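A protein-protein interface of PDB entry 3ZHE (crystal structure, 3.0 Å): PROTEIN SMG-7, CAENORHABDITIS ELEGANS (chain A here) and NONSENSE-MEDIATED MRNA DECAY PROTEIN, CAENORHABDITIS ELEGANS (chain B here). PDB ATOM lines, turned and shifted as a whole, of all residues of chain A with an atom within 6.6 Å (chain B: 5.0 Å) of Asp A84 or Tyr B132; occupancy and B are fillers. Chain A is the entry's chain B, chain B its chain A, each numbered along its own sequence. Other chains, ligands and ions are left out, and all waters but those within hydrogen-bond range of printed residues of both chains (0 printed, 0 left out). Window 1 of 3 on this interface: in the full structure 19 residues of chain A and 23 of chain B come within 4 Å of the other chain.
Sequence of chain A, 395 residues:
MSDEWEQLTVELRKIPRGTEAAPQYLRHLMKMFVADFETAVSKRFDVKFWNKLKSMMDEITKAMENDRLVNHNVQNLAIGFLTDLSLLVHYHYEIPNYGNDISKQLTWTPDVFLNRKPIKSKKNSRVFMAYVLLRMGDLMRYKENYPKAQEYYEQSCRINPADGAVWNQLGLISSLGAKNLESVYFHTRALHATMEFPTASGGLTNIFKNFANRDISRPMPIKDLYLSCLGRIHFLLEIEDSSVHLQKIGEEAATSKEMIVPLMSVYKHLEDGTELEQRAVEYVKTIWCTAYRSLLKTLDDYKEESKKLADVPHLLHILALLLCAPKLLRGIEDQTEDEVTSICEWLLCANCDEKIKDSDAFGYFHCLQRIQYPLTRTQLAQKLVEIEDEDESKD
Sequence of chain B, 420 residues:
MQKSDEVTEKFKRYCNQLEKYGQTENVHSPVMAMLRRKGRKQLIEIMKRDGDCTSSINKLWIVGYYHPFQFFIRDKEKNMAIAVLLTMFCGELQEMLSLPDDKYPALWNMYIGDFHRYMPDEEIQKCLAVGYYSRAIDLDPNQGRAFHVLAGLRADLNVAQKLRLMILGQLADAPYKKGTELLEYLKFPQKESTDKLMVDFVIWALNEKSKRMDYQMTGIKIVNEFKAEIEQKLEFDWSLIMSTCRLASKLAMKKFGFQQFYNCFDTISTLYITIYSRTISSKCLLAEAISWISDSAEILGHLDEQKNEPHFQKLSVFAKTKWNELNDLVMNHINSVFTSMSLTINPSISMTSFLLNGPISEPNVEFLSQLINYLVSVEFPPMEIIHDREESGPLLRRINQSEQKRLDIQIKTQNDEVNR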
ATOM      1  N   MET A  30      -5.918 -26.781 -10.069  1.00  0.00           N
ATOM      2  CA  MET A  30      -6.238 -25.740 -11.042  1.00  0.00           C
ATOM      3  C   MET A  30      -5.334 -24.528 -10.842  1.00  0.00           C
ATOM      4  O   MET A  30      -4.805 -23.961 -11.808  1.00  0.00           O
ATOM      5  CB  MET A  30      -7.704 -25.321 -10.921  1.00  0.00           C
ATOM      6  CG  MET A  30      -8.691 -26.324 -11.490  1.00  0.00           C
ATOM      7  SD  MET A  30     -10.394 -25.899 -11.083  1.00  0.00           S
ATOM      8  CE  MET A  30     -11.284 -26.924 -12.248  1.00  0.00           C
ATOM      9  N   PHE A  49      -5.337 -34.939 -11.505  1.00  0.00           N
ATOM     10  CA  PHE A  49      -6.657 -34.321 -11.518  1.00  0.00           C
ATOM     11  C   PHE A  49      -7.722 -35.376 -11.781  1.00  0.00           C
ATOM     12  O   PHE A  49      -8.654 -35.559 -10.984  1.00  0.00           O
ATOM     13  CB  PHE A  49      -6.705 -33.255 -12.616  1.00  0.00           C
ATOM     14  CG  PHE A  49      -7.905 -32.354 -12.548  1.00  0.00           C
ATOM     15  CD1 PHE A  49      -9.093 -32.706 -13.170  1.00  0.00           C
ATOM     16  CD2 PHE A  49      -7.839 -31.142 -11.879  1.00  0.00           C
ATOM     17  CE1 PHE A  49     -10.197 -31.872 -13.114  1.00  0.00           C
ATOM     18  CE2 PHE A  49      -8.938 -30.304 -11.820  1.00  0.00           C
ATOM     19  CZ  PHE A  49     -10.118 -30.669 -12.438  1.00  0.00           C
ATOM     20  N   ILE A  79     -18.069 -33.284 -14.898  1.00  0.00           N
ATOM     21  CA  ILE A  79     -18.099 -32.566 -16.171  1.00  0.00           C
ATOM     22  C   ILE A  79     -17.761 -31.093 -15.970  1.00  0.00           C
ATOM     23  O   ILE A  79     -16.940 -30.524 -16.702  1.00  0.00           O
ATOM     24  CB  ILE A  79     -19.480 -32.680 -16.851  1.00  0.00           C
ATOM     25  CG1 ILE A  79     -19.754 -34.124 -17.279  1.00  0.00           C
ATOM     26  CG2 ILE A  79     -19.568 -31.745 -18.048  1.00  0.00           C
ATOM     27  CD1 ILE A  79     -21.115 -34.321 -17.916  1.00  0.00           C
ATOM     28  N   GLY A  80     -18.388 -30.488 -14.964  1.00  0.00           N
ATOM     29  CA  GLY A  80     -18.113 -29.106 -14.616  1.00  0.00           C
ATOM     30  C   GLY A  80     -16.647 -28.865 -14.308  1.00  0.00           C
ATOM     31  O   GLY A  80     -16.022 -27.971 -14.888  1.00  0.00           O
ATOM     32  N   PHE A  81     -16.094 -29.669 -13.404  1.00  0.00           N
ATOM     33  CA  PHE A  81     -14.691 -29.527 -13.020  1.00  0.00           C
ATOM     34  C   PHE A  81     -13.733 -29.630 -14.211  1.00  0.00           C
ATOM     35  O   PHE A  81     -12.848 -28.788 -14.378  1.00  0.00           O
ATOM     36  CB  PHE A  81     -14.311 -30.548 -11.942  1.00  0.00           C
ATOM     37  CG  PHE A  81     -14.356 -30.001 -10.543  1.00  0.00           C
ATOM     38  CD1 PHE A  81     -13.377 -29.128 -10.094  1.00  0.00           C
ATOM     39  CD2 PHE A  81     -15.366 -30.371  -9.672  1.00  0.00           C
ATOM     40  CE1 PHE A  81     -13.415 -28.628  -8.806  1.00  0.00           C
ATOM     41  CE2 PHE A  81     -15.406 -29.875  -8.381  1.00  0.00           C
ATOM     42  CZ  PHE A  81     -14.430 -29.002  -7.949  1.00  0.00           C
ATOM     43  N   LEU A  82     -13.917 -30.653 -15.040  1.00  0.00           N
ATOM     44  CA  LEU A  82     -13.021 -30.868 -16.175  1.00  0.00           C
ATOM     45  C   LEU A  82     -13.129 -29.753 -17.217  1.00  0.00           C
ATOM     46  O   LEU A  82     -12.109 -29.238 -17.697  1.00  0.00           O
ATOM     47  CB  LEU A  82     -13.287 -32.228 -16.820  1.00  0.00           C
ATOM     48  CG  LEU A  82     -12.195 -32.770 -17.743  1.00  0.00           C
ATOM     49  CD1 LEU A  82     -10.854 -32.774 -17.029  1.00  0.00           C
ATOM     50  CD2 LEU A  82     -12.551 -34.171 -18.210  1.00  0.00           C
ATOM     51  N   THR A  83     -14.361 -29.386 -17.564  1.00  0.00           N
ATOM     52  CA  THR A  83     -14.590 -28.296 -18.508  1.00  0.00           C
ATOM     53  C   THR A  83     -13.916 -27.018 -18.020  1.00  0.00           C
ATOM     54  O   THR A  83     -13.202 -26.344 -18.774  1.00  0.00           O
ATOM     55  CB  THR A  83     -16.095 -28.039 -18.716  1.00  0.00           C
ATOM     56  OG1 THR A  83     -16.671 -29.136 -19.432  1.00  0.00           O
ATOM     57  CG2 THR A  83     -16.321 -26.761 -19.505  1.00  0.00           C
ATOM     58  N   ASP A  84     -14.132 -26.703 -16.747  1.00  0.00           N
ATOM     59  CA  ASP A  84     -13.528 -25.519 -16.153  1.00  0.00           C
ATOM     60  C   ASP A  84     -12.006 -25.600 -16.128  1.00  0.00           C
ATOM     61  O   ASP A  84     -11.330 -24.580 -16.223  1.00  0.00           O
ATOM     62  CB  ASP A  84     -14.086 -25.259 -14.752  1.00  0.00           C
ATOM     63  CG  ASP A  84     -15.474 -24.656 -14.789  1.00  0.00           C
ATOM     64  OD1 ASP A  84     -15.888 -24.196 -15.874  1.00  0.00           O
ATOM     65  OD2 ASP A  84     -16.145 -24.630 -13.735  1.00  0.00           O
ATOM     66  N   LEU A  85     -11.470 -26.812 -16.007  1.00  0.00           N
ATOM     67  CA  LEU A  85     -10.026 -27.011 -16.094  1.00  0.00           C
ATOM     68  C   LEU A  85      -9.519 -26.613 -17.474  1.00  0.00           C
ATOM     69  O   LEU A  85      -8.583 -25.814 -17.599  1.00  0.00           O
ATOM     70  CB  LEU A  85      -9.657 -28.467 -15.804  1.00  0.00           C
ATOM     71  CG  LEU A  85      -8.190 -28.841 -16.035  1.00  0.00           C
ATOM     72  CD1 LEU A  85      -7.267 -28.069 -15.100  1.00  0.00           C
ATOM     73  CD2 LEU A  85      -7.984 -30.341 -15.878  1.00  0.00           C
ATOM     74  N   SER A  86     -10.149 -27.172 -18.507  1.00  0.00           N
ATOM     75  CA  SER A  86      -9.760 -26.877 -19.885  1.00  0.00           C
ATOM     76  C   SER A  86      -9.825 -25.380 -20.170  1.00  0.00           C
ATOM     77  O   SER A  86      -8.878 -24.793 -20.708  1.00  0.00           O
ATOM     78  CB  SER A  86     -10.658 -27.628 -20.870  1.00  0.00           C
ATOM     79  OG  SER A  86     -10.309 -27.326 -22.210  1.00  0.00           O
ATOM     80  N   LEU A  87     -10.943 -24.766 -19.798  1.00  0.00           N
ATOM     81  CA  LEU A  87     -11.146 -23.340 -20.035  1.00  0.00           C
ATOM     82  C   LEU A  87     -10.163 -22.465 -19.261  1.00  0.00           C
ATOM     83  O   LEU A  87      -9.680 -21.455 -19.774  1.00  0.00           O
ATOM     84  CB  LEU A  87     -12.584 -22.944 -19.707  1.00  0.00           C
ATOM     85  CG  LEU A  87     -13.627 -23.538 -20.652  1.00  0.00           C
ATOM     86  CD1 LEU A  87     -15.018 -23.051 -20.290  1.00  0.00           C
ATOM     87  CD2 LEU A  87     -13.284 -23.178 -22.085  1.00  0.00           C
ATOM     88  N   LEU A  88      -9.872 -22.855 -18.024  1.00  0.00           N
ATOM     89  CA  LEU A  88      -8.905 -22.135 -17.205  1.00  0.00           C
ATOM     90  C   LEU A  88      -7.511 -22.222 -17.809  1.00  0.00           C
ATOM     91  O   LEU A  88      -6.732 -21.271 -17.725  1.00  0.00           O
ATOM     92  CB  LEU A  88      -8.893 -22.657 -15.767  1.00  0.00           C
ATOM     93  CG  LEU A  88      -9.865 -21.990 -14.793  1.00  0.00           C
ATOM     94  CD1 LEU A  88      -9.783 -22.635 -13.419  1.00  0.00           C
ATOM     95  CD2 LEU A  88      -9.577 -20.501 -14.704  1.00  0.00           C
ATOM     96  N   VAL A  89      -7.196 -23.362 -18.416  1.00  0.00           N
ATOM     97  CA  VAL A  89      -5.926 -23.499 -19.121  1.00  0.00           C
ATOM     98  C   VAL A  89      -5.885 -22.594 -20.352  1.00  0.00           C
ATOM     99  O   VAL A  89      -4.902 -21.884 -20.572  1.00  0.00           O
ATOM    100  CB  VAL A  89      -5.635 -24.962 -19.510  1.00  0.00           C
ATOM    101  CG1 VAL A  89      -4.603 -25.021 -20.627  1.00  0.00           C
ATOM    102  CG2 VAL A  89      -5.159 -25.738 -18.293  1.00  0.00           C
ATOM    103  N   TYR A  91      -7.582 -19.894 -20.886  1.00  0.00           N
ATOM    104  CA  TYR A  91      -7.667 -18.502 -20.450  1.00  0.00           C
ATOM    105  C   TYR A  91      -6.300 -17.857 -20.216  1.00  0.00           C
ATOM    106  O   TYR A  91      -6.148 -16.642 -20.350  1.00  0.00           O
ATOM    107  CB  TYR A  91      -8.498 -18.433 -19.166  1.00  0.00           C
ATOM    108  CG  TYR A  91      -8.952 -17.048 -18.759  1.00  0.00           C
ATOM    109  CD1 TYR A  91     -10.151 -16.527 -19.226  1.00  0.00           C
ATOM    110  CD2 TYR A  91      -8.196 -16.275 -17.887  1.00  0.00           C
ATOM    111  CE1 TYR A  91     -10.579 -15.270 -18.850  1.00  0.00           C
ATOM    112  CE2 TYR A  91      -8.614 -15.015 -17.505  1.00  0.00           C
ATOM    113  CZ  TYR A  91      -9.807 -14.518 -17.989  1.00  0.00           C
ATOM    114  OH  TYR A  91     -10.228 -13.264 -17.611  1.00  0.00           O
ATOM    115  N   GLN A 105     -16.992 -25.623 -26.077  1.00  0.00           N
ATOM    116  CA  GLN A 105     -17.225 -25.483 -24.643  1.00  0.00           C
ATOM    117  C   GLN A 105     -15.940 -25.715 -23.856  1.00  0.00           C
ATOM    118  O   GLN A 105     -15.769 -25.190 -22.756  1.00  0.00           O
ATOM    119  CB  GLN A 105     -18.308 -26.454 -24.175  1.00  0.00           C
ATOM    120  CG  GLN A 105     -19.684 -26.153 -24.735  1.00  0.00           C
ATOM    121  CD  GLN A 105     -20.135 -27.170 -25.763  1.00  0.00           C
ATOM    122  OE1 GLN A 105     -19.918 -28.372 -25.603  1.00  0.00           O
ATOM    123  NE2 GLN A 105     -20.767 -26.693 -26.828  1.00  0.00           N
ATOM    124  N   LEU A 106     -15.044 -26.512 -24.428  1.00  0.00           N
ATOM    125  CA  LEU A 106     -13.744 -26.755 -23.824  1.00  0.00           C
ATOM    126  C   LEU A 106     -12.737 -25.789 -24.421  1.00  0.00           C
ATOM    127  O   LEU A 106     -11.674 -25.549 -23.850  1.00  0.00           O
ATOM    128  CB  LEU A 106     -13.281 -28.183 -24.109  1.00  0.00           C
ATOM    129  CG  LEU A 106     -14.299 -29.318 -23.995  1.00  0.00           C
ATOM    130  CD1 LEU A 106     -13.636 -30.636 -24.349  1.00  0.00           C
ATOM    131  CD2 LEU A 106     -14.899 -29.376 -22.601  1.00  0.00           C
ATOM    132  N   TRP A 108     -13.608 -22.566 -26.598  1.00  0.00           N
ATOM    133  CA  TRP A 108     -13.939 -21.179 -26.928  1.00  0.00           C
ATOM    134  C   TRP A 108     -13.208 -20.763 -28.199  1.00  0.00           C
ATOM    135  O   TRP A 108     -12.922 -21.598 -29.056  1.00  0.00           O
ATOM    136  CB  TRP A 108     -13.629 -20.222 -25.773  1.00  0.00           C
ATOM    137  CG  TRP A 108     -14.630 -20.288 -24.663  1.00  0.00           C
ATOM    138  CD1 TRP A 108     -15.887 -20.819 -24.722  1.00  0.00           C
ATOM    139  CD2 TRP A 108     -14.458 -19.811 -23.322  1.00  0.00           C
ATOM    140  NE1 TRP A 108     -16.508 -20.698 -23.500  1.00  0.00           N
ATOM    141  CE2 TRP A 108     -15.651 -20.084 -22.625  1.00  0.00           C
ATOM    142  CE3 TRP A 108     -13.409 -19.179 -22.646  1.00  0.00           C
ATOM    143  CZ2 TRP A 108     -15.825 -19.746 -21.282  1.00  0.00           C
ATOM    144  CZ3 TRP A 108     -13.583 -18.845 -21.313  1.00  0.00           C
ATOM    145  CH2 TRP A 108     -14.782 -19.128 -20.645  1.00  0.00           C
ATOM    146  N   THR B  87     -20.239 -25.295  -9.452  1.00  0.00           N
ATOM    147  CA  THR B  87     -19.574 -26.121 -10.455  1.00  0.00           C
ATOM    148  C   THR B  87     -20.484 -27.249 -10.936  1.00  0.00           C
ATOM    149  O   THR B  87     -20.578 -27.517 -12.137  1.00  0.00           O
ATOM    150  CB  THR B  87     -18.253 -26.708  -9.922  1.00  0.00           C
ATOM    151  OG1 THR B  87     -17.371 -25.643  -9.549  1.00  0.00           O
ATOM    152  CG2 THR B  87     -17.582 -27.563 -10.984  1.00  0.00           C
ATOM    153  N   CYS B  90     -22.914 -25.905 -13.215  1.00  0.00           N
ATOM    154  CA  CYS B  90     -22.287 -25.631 -14.504  1.00  0.00           C
ATOM    155  C   CYS B  90     -22.205 -26.885 -15.362  1.00  0.00           C
ATOM    156  O   CYS B  90     -22.552 -26.862 -16.543  1.00  0.00           O
ATOM    157  CB  CYS B  90     -20.886 -25.049 -14.315  1.00  0.00           C
ATOM    158  SG  CYS B  90     -20.852 -23.412 -13.563  1.00  0.00           S
ATOM    159  N   GLN B  94     -24.109 -27.653 -18.861  1.00  0.00           N
ATOM    160  CA  GLN B  94     -23.217 -27.852 -20.000  1.00  0.00           C
ATOM    161  C   GLN B  94     -23.866 -28.783 -21.026  1.00  0.00           C
ATOM    162  O   GLN B  94     -23.465 -28.817 -22.192  1.00  0.00           O
ATOM    163  CB  GLN B  94     -21.872 -28.418 -19.533  1.00  0.00           C
ATOM    164  CG  GLN B  94     -20.682 -28.057 -20.422  1.00  0.00           C
ATOM    165  CD  GLN B  94     -20.080 -26.703 -20.083  1.00  0.00           C
ATOM    166  OE1 GLN B  94     -20.285 -26.176 -18.989  1.00  0.00           O
ATOM    167  NE2 GLN B  94     -19.332 -26.134 -21.023  1.00  0.00           N
ATOM    168  N   ASN B 109     -24.358 -19.846 -22.260  1.00  0.00           N
ATOM    169  CA  ASN B 109     -23.040 -19.326 -21.918  1.00  0.00           C
ATOM    170  C   ASN B 109     -23.118 -18.189 -20.897  1.00  0.00           C
ATOM    171  O   ASN B 109     -22.272 -18.079 -20.011  1.00  0.00           O
ATOM    172  CB  ASN B 109     -22.275 -18.885 -23.173  1.00  0.00           C
ATOM    173  CG  ASN B 109     -21.584 -20.046 -23.875  1.00  0.00           C
ATOM    174  OD1 ASN B 109     -22.110 -20.613 -24.832  1.00  0.00           O
ATOM    175  ND2 ASN B 109     -20.397 -20.403 -23.395  1.00  0.00           N
ATOM    176  N   ILE B 112     -24.115 -19.837 -17.396  1.00  0.00           N
ATOM    177  CA  ILE B 112     -22.945 -20.458 -16.790  1.00  0.00           C
ATOM    178  C   ILE B 112     -21.982 -19.362 -16.337  1.00  0.00           C
ATOM    179  O   ILE B 112     -21.368 -19.457 -15.270  1.00  0.00           O
ATOM    180  CB  ILE B 112     -22.258 -21.448 -17.753  1.00  0.00           C
ATOM    181  CG1 ILE B 112     -23.254 -22.525 -18.193  1.00  0.00           C
ATOM    182  CG2 ILE B 112     -21.049 -22.093 -17.091  1.00  0.00           C
ATOM    183  CD1 ILE B 112     -22.674 -23.575 -19.120  1.00  0.00           C
ATOM    184  N   GLY B 113     -21.881 -18.309 -17.143  1.00  0.00           N
ATOM    185  CA  GLY B 113     -21.107 -17.135 -16.781  1.00  0.00           C
ATOM    186  C   GLY B 113     -21.602 -16.512 -15.490  1.00  0.00           C
ATOM    187  O   GLY B 113     -20.802 -16.071 -14.662  1.00  0.00           O
ATOM    188  N   HIS B 116     -20.379 -18.669 -12.633  1.00  0.00           N
ATOM    189  CA  HIS B 116     -18.995 -18.361 -12.297  1.00  0.00           C
ATOM    190  C   HIS B 116     -18.865 -16.994 -11.622  1.00  0.00           C
ATOM    191  O   HIS B 116     -17.957 -16.778 -10.820  1.00  0.00           O
ATOM    192  CB  HIS B 116     -18.100 -18.447 -13.535  1.00  0.00           C
ATOM    193  CG  HIS B 116     -17.831 -19.848 -13.992  1.00  0.00           C
ATOM    194  ND1 HIS B 116     -18.780 -20.623 -14.622  1.00  0.00           N
ATOM    195  CD2 HIS B 116     -16.717 -20.612 -13.907  1.00  0.00           C
ATOM    196  CE1 HIS B 116     -18.261 -21.804 -14.909  1.00  0.00           C
ATOM    197  NE2 HIS B 116     -17.011 -21.823 -14.484  1.00  0.00           N
ATOM    198  N   MET B 119     -19.571 -17.112  -7.746  1.00  0.00           N
ATOM    199  CA  MET B 119     -18.529 -17.695  -6.910  1.00  0.00           C
ATOM    200  C   MET B 119     -17.843 -16.632  -6.061  1.00  0.00           C
ATOM    201  O   MET B 119     -17.679 -15.493  -6.502  1.00  0.00           O
ATOM    202  CB  MET B 119     -17.497 -18.424  -7.773  1.00  0.00           C
ATOM    203  CG  MET B 119     -18.057 -19.617  -8.528  1.00  0.00           C
ATOM    204  SD  MET B 119     -16.786 -20.614  -9.322  1.00  0.00           S
ATOM    205  CE  MET B 119     -17.786 -21.897 -10.071  1.00  0.00           C
ATOM    206  N   GLN B 125     -11.738 -20.409 -10.299  1.00  0.00           N
ATOM    207  CA  GLN B 125     -12.797 -20.658 -11.278  1.00  0.00           C
ATOM    208  C   GLN B 125     -13.601 -19.409 -11.641  1.00  0.00           C
ATOM    209  O   GLN B 125     -14.291 -19.383 -12.660  1.00  0.00           O
ATOM    210  CB  GLN B 125     -13.752 -21.745 -10.770  1.00  0.00           C
ATOM    211  CG  GLN B 125     -13.120 -23.116 -10.562  1.00  0.00           C
ATOM    212  CD  GLN B 125     -14.121 -24.151 -10.069  1.00  0.00           C
ATOM    213  OE1 GLN B 125     -14.089 -24.558  -8.908  1.00  0.00           O
ATOM    214  NE2 GLN B 125     -15.012 -24.585 -10.955  1.00  0.00           N
ATOM    215  N   LEU B 128     -13.119 -17.524 -15.329  1.00  0.00           N
ATOM    216  CA  LEU B 128     -13.905 -17.980 -16.472  1.00  0.00           C
ATOM    217  C   LEU B 128     -15.174 -17.172 -16.716  1.00  0.00           C
ATOM    218  O   LEU B 128     -15.635 -17.080 -17.859  1.00  0.00           O
ATOM    219  CB  LEU B 128     -14.258 -19.458 -16.308  1.00  0.00           C
ATOM    220  CG  LEU B 128     -13.060 -20.396 -16.171  1.00  0.00           C
ATOM    221  CD1 LEU B 128     -13.518 -21.840 -16.069  1.00  0.00           C
ATOM    222  CD2 LEU B 128     -12.119 -20.209 -17.346  1.00  0.00           C
ATOM    223  N   ALA B 129     -15.721 -16.592 -15.644  1.00  0.00           N
ATOM    224  CA  ALA B 129     -16.908 -15.746 -15.752  1.00  0.00           C
ATOM    225  C   ALA B 129     -16.763 -14.801 -16.925  1.00  0.00           C
ATOM    226  O   ALA B 129     -17.552 -14.870 -17.876  1.00  0.00           O
ATOM    227  CB  ALA B 129     -17.147 -14.964 -14.476  1.00  0.00           C
ATOM    228  N   VAL B 130     -15.730 -13.959 -16.868  1.00  0.00           N
ATOM    229  CA  VAL B 130     -15.459 -13.001 -17.934  1.00  0.00           C
ATOM    230  C   VAL B 130     -15.526 -13.720 -19.267  1.00  0.00           C
ATOM    231  O   VAL B 130     -16.359 -13.395 -20.124  1.00  0.00           O
ATOM    232  CB  VAL B 130     -14.066 -12.359 -17.778  1.00  0.00           C
ATOM    233  CG1 VAL B 130     -13.666 -11.643 -19.057  1.00  0.00           C
ATOM    234  CG2 VAL B 130     -14.049 -11.406 -16.590  1.00  0.00           C
ATOM    235  N   GLY B 131     -14.687 -14.747 -19.395  1.00  0.00           N
ATOM    236  CA  GLY B 131     -14.588 -15.522 -20.615  1.00  0.00           C
ATOM    237  C   GLY B 131     -15.949 -15.942 -21.121  1.00  0.00           C
ATOM    238  O   GLY B 131     -16.275 -15.712 -22.289  1.00  0.00           O
ATOM    239  N   TYR B 132     -16.760 -16.513 -20.233  1.00  0.00           N
ATOM    240  CA  TYR B 132     -18.068 -17.013 -20.638  1.00  0.00           C
ATOM    241  C   TYR B 132     -18.887 -15.922 -21.309  1.00  0.00           C
ATOM    242  O   TYR B 132     -19.406 -16.124 -22.412  1.00  0.00           O
ATOM    243  CB  TYR B 132     -18.825 -17.630 -19.460  1.00  0.00           C
ATOM    244  CG  TYR B 132     -18.602 -19.118 -19.318  1.00  0.00           C
ATOM    245  CD1 TYR B 132     -19.272 -20.019 -20.135  1.00  0.00           C
ATOM    246  CD2 TYR B 132     -17.718 -19.622 -18.373  1.00  0.00           C
ATOM    247  CE1 TYR B 132     -19.070 -21.380 -20.014  1.00  0.00           C
ATOM    248  CE2 TYR B 132     -17.509 -20.983 -18.244  1.00  0.00           C
ATOM    249  CZ  TYR B 132     -18.188 -21.857 -19.068  1.00  0.00           C
ATOM    250  OH  TYR B 132     -17.987 -23.213 -18.945  1.00  0.00           O
ATOM    251  N   TYR B 133     -18.961 -14.757 -20.670  1.00  0.00           N
ATOM    252  CA  TYR B 133     -19.742 -13.663 -21.227  1.00  0.00           C
ATOM    253  C   TYR B 133     -19.211 -13.315 -22.608  1.00  0.00           C
ATOM    254  O   TYR B 133     -19.990 -13.159 -23.554  1.00  0.00           O
ATOM    255  CB  TYR B 133     -19.732 -12.445 -20.302  1.00  0.00           C
ATOM    256  CG  TYR B 133     -20.525 -12.661 -19.036  1.00  0.00           C
ATOM    257  CD1 TYR B 133     -21.908 -12.785 -19.076  1.00  0.00           C
ATOM    258  CD2 TYR B 133     -19.893 -12.751 -17.804  1.00  0.00           C
ATOM    259  CE1 TYR B 133     -22.638 -12.990 -17.924  1.00  0.00           C
ATOM    260  CE2 TYR B 133     -20.616 -12.957 -16.647  1.00  0.00           C
ATOM    261  CZ  TYR B 133     -21.987 -13.074 -16.711  1.00  0.00           C
ATOM    262  OH  TYR B 133     -22.703 -13.277 -15.555  1.00  0.00           O
ATOM    263  N   SER B 134     -17.885 -13.256 -22.727  1.00  0.00           N
ATOM    264  CA  SER B 134     -17.253 -12.956 -24.001  1.00  0.00           C
ATOM    265  C   SER B 134     -17.751 -13.945 -25.045  1.00  0.00           C
ATOM    266  O   SER B 134     -18.186 -13.549 -26.131  1.00  0.00           O
ATOM    267  CB  SER B 134     -15.733 -13.030 -23.879  1.00  0.00           C
ATOM    268  OG  SER B 134     -15.259 -12.186 -22.848  1.00  0.00           O
ATOM    269  N   ARG B 135     -17.728 -15.227 -24.683  1.00  0.00           N
ATOM    270  CA  ARG B 135     -18.179 -16.281 -25.583  1.00  0.00           C
ATOM    271  C   ARG B 135     -19.601 -16.007 -26.046  1.00  0.00           C
ATOM    272  O   ARG B 135     -19.898 -16.099 -27.239  1.00  0.00           O
ATOM    273  CB  ARG B 135     -18.088 -17.652 -24.910  1.00  0.00           C
ATOM    274  CG  ARG B 135     -18.684 -18.785 -25.730  1.00  0.00           C
ATOM    275  CD  ARG B 135     -18.033 -18.889 -27.100  1.00  0.00           C
ATOM    276  NE  ARG B 135     -18.641 -19.940 -27.912  1.00  0.00           N
ATOM    277  CZ  ARG B 135     -18.348 -20.159 -29.191  1.00  0.00           C
ATOM    278  NH1 ARG B 135     -17.454 -19.398 -29.809  1.00  0.00           N
ATOM    279  NH2 ARG B 135     -18.951 -21.138 -29.852  1.00  0.00           N
ATOM    280  N   ALA B 136     -20.464 -15.635 -25.103  1.00  0.00           N
ATOM    281  CA  ALA B 136     -21.852 -15.344 -25.428  1.00  0.00           C
ATOM    282  C   ALA B 136     -21.904 -14.273 -26.506  1.00  0.00           C
ATOM    283  O   ALA B 136     -22.614 -14.415 -27.501  1.00  0.00           O
ATOM    284  CB  ALA B 136     -22.610 -14.900 -24.196  1.00  0.00           C
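The side-chain amide nitrogen of Gln B125 lies within hydrogen-bond range of the side-chain carboxylate of Asp A84, at 3.0 Å.
NE2 of His B116 lies within hydrogen-bond range of OD1 of Asp A84 (3.0 Å).
OG1 of Thr A83 lies within hydrogen-bond range of O of Ile A79, at 3.1 Å.
OE1 of Gln B94 sits close to O of Cys B90.
O of Val B130 lies within hydrogen-bond range of OG of Ser B134.
OG1 of Thr B87 sits at hydrogen-bond distance from NE2 of Gln B125, 2.9 Å away.
The side-chain sulfur (SG) of Cys B90 sits close to a ring nitrogen (ND1) of His B116.
The backbone carbonyl oxygen (O) of Ile B112 sits at hydrogen-bond distance from a ring nitrogen (ND1) of His B116 (2.9 Å).
Among the printed residues, pairs that only touch across the chains: Leu A87 with Tyr B132 (3.3 Å), Trp A108 with Tyr B132 (3.3 Å), Gln A105 with Gln B94 (3.3 Å), Asp A84 with Leu B128 (3.3 Å), Trp A108 with Gly B131 (3.4 Å), Thr A83 with Gln B94 (3.4 Å), Phe A81 with Thr B87 (3.5 Å), Leu A88 with Leu B128 (3.5 Å), Leu A87 with Leu B128 (3.5 Å), Trp A108 with Leu B128 (3.6 Å), Trp A108 with Arg B135 (3.6 Å), Gly A80 with Thr B87 (3.7 Å), Asp A84 with Tyr B132 (3.8 Å), Trp A108 with Asn B109 (3.9 Å), Met A30 with Gln B125 (3.9 Å), Tyr A91 with Val B130 (3.9 Å) and Thr A83 with Tyr B132 (3.96 Å).
Asp A84 touches just these residues of chain B: His B116 (3.0 Å), Gln B125 (3.0 Å), Leu B128 (3.3 Å) and Tyr B132 (3.8 Å).
Printed residues of chain A within 4 Å of Thr B87: Gly A80 and Phe A81.
Printed residues of chain A within 4 Å of Asn B109: Trp A108.
Of the printed residues of chain A, Gln B125 touches Met A30 and Asp A84.
Of chain A, only Thr A83 (3.96 Å), Asp A84 (3.8 Å), Leu A87 (3.3 Å) and Trp A108 (3.3 Å) come within 4 Å of Tyr B132.
Along chain B the printed residues that touch a printed residue of chain A span positions 87 to 135.
Among the printed residues, no Asp or Glu carboxylate lies within 4 Å of a Lys or Arg side-chain nitrogen of the other chain.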
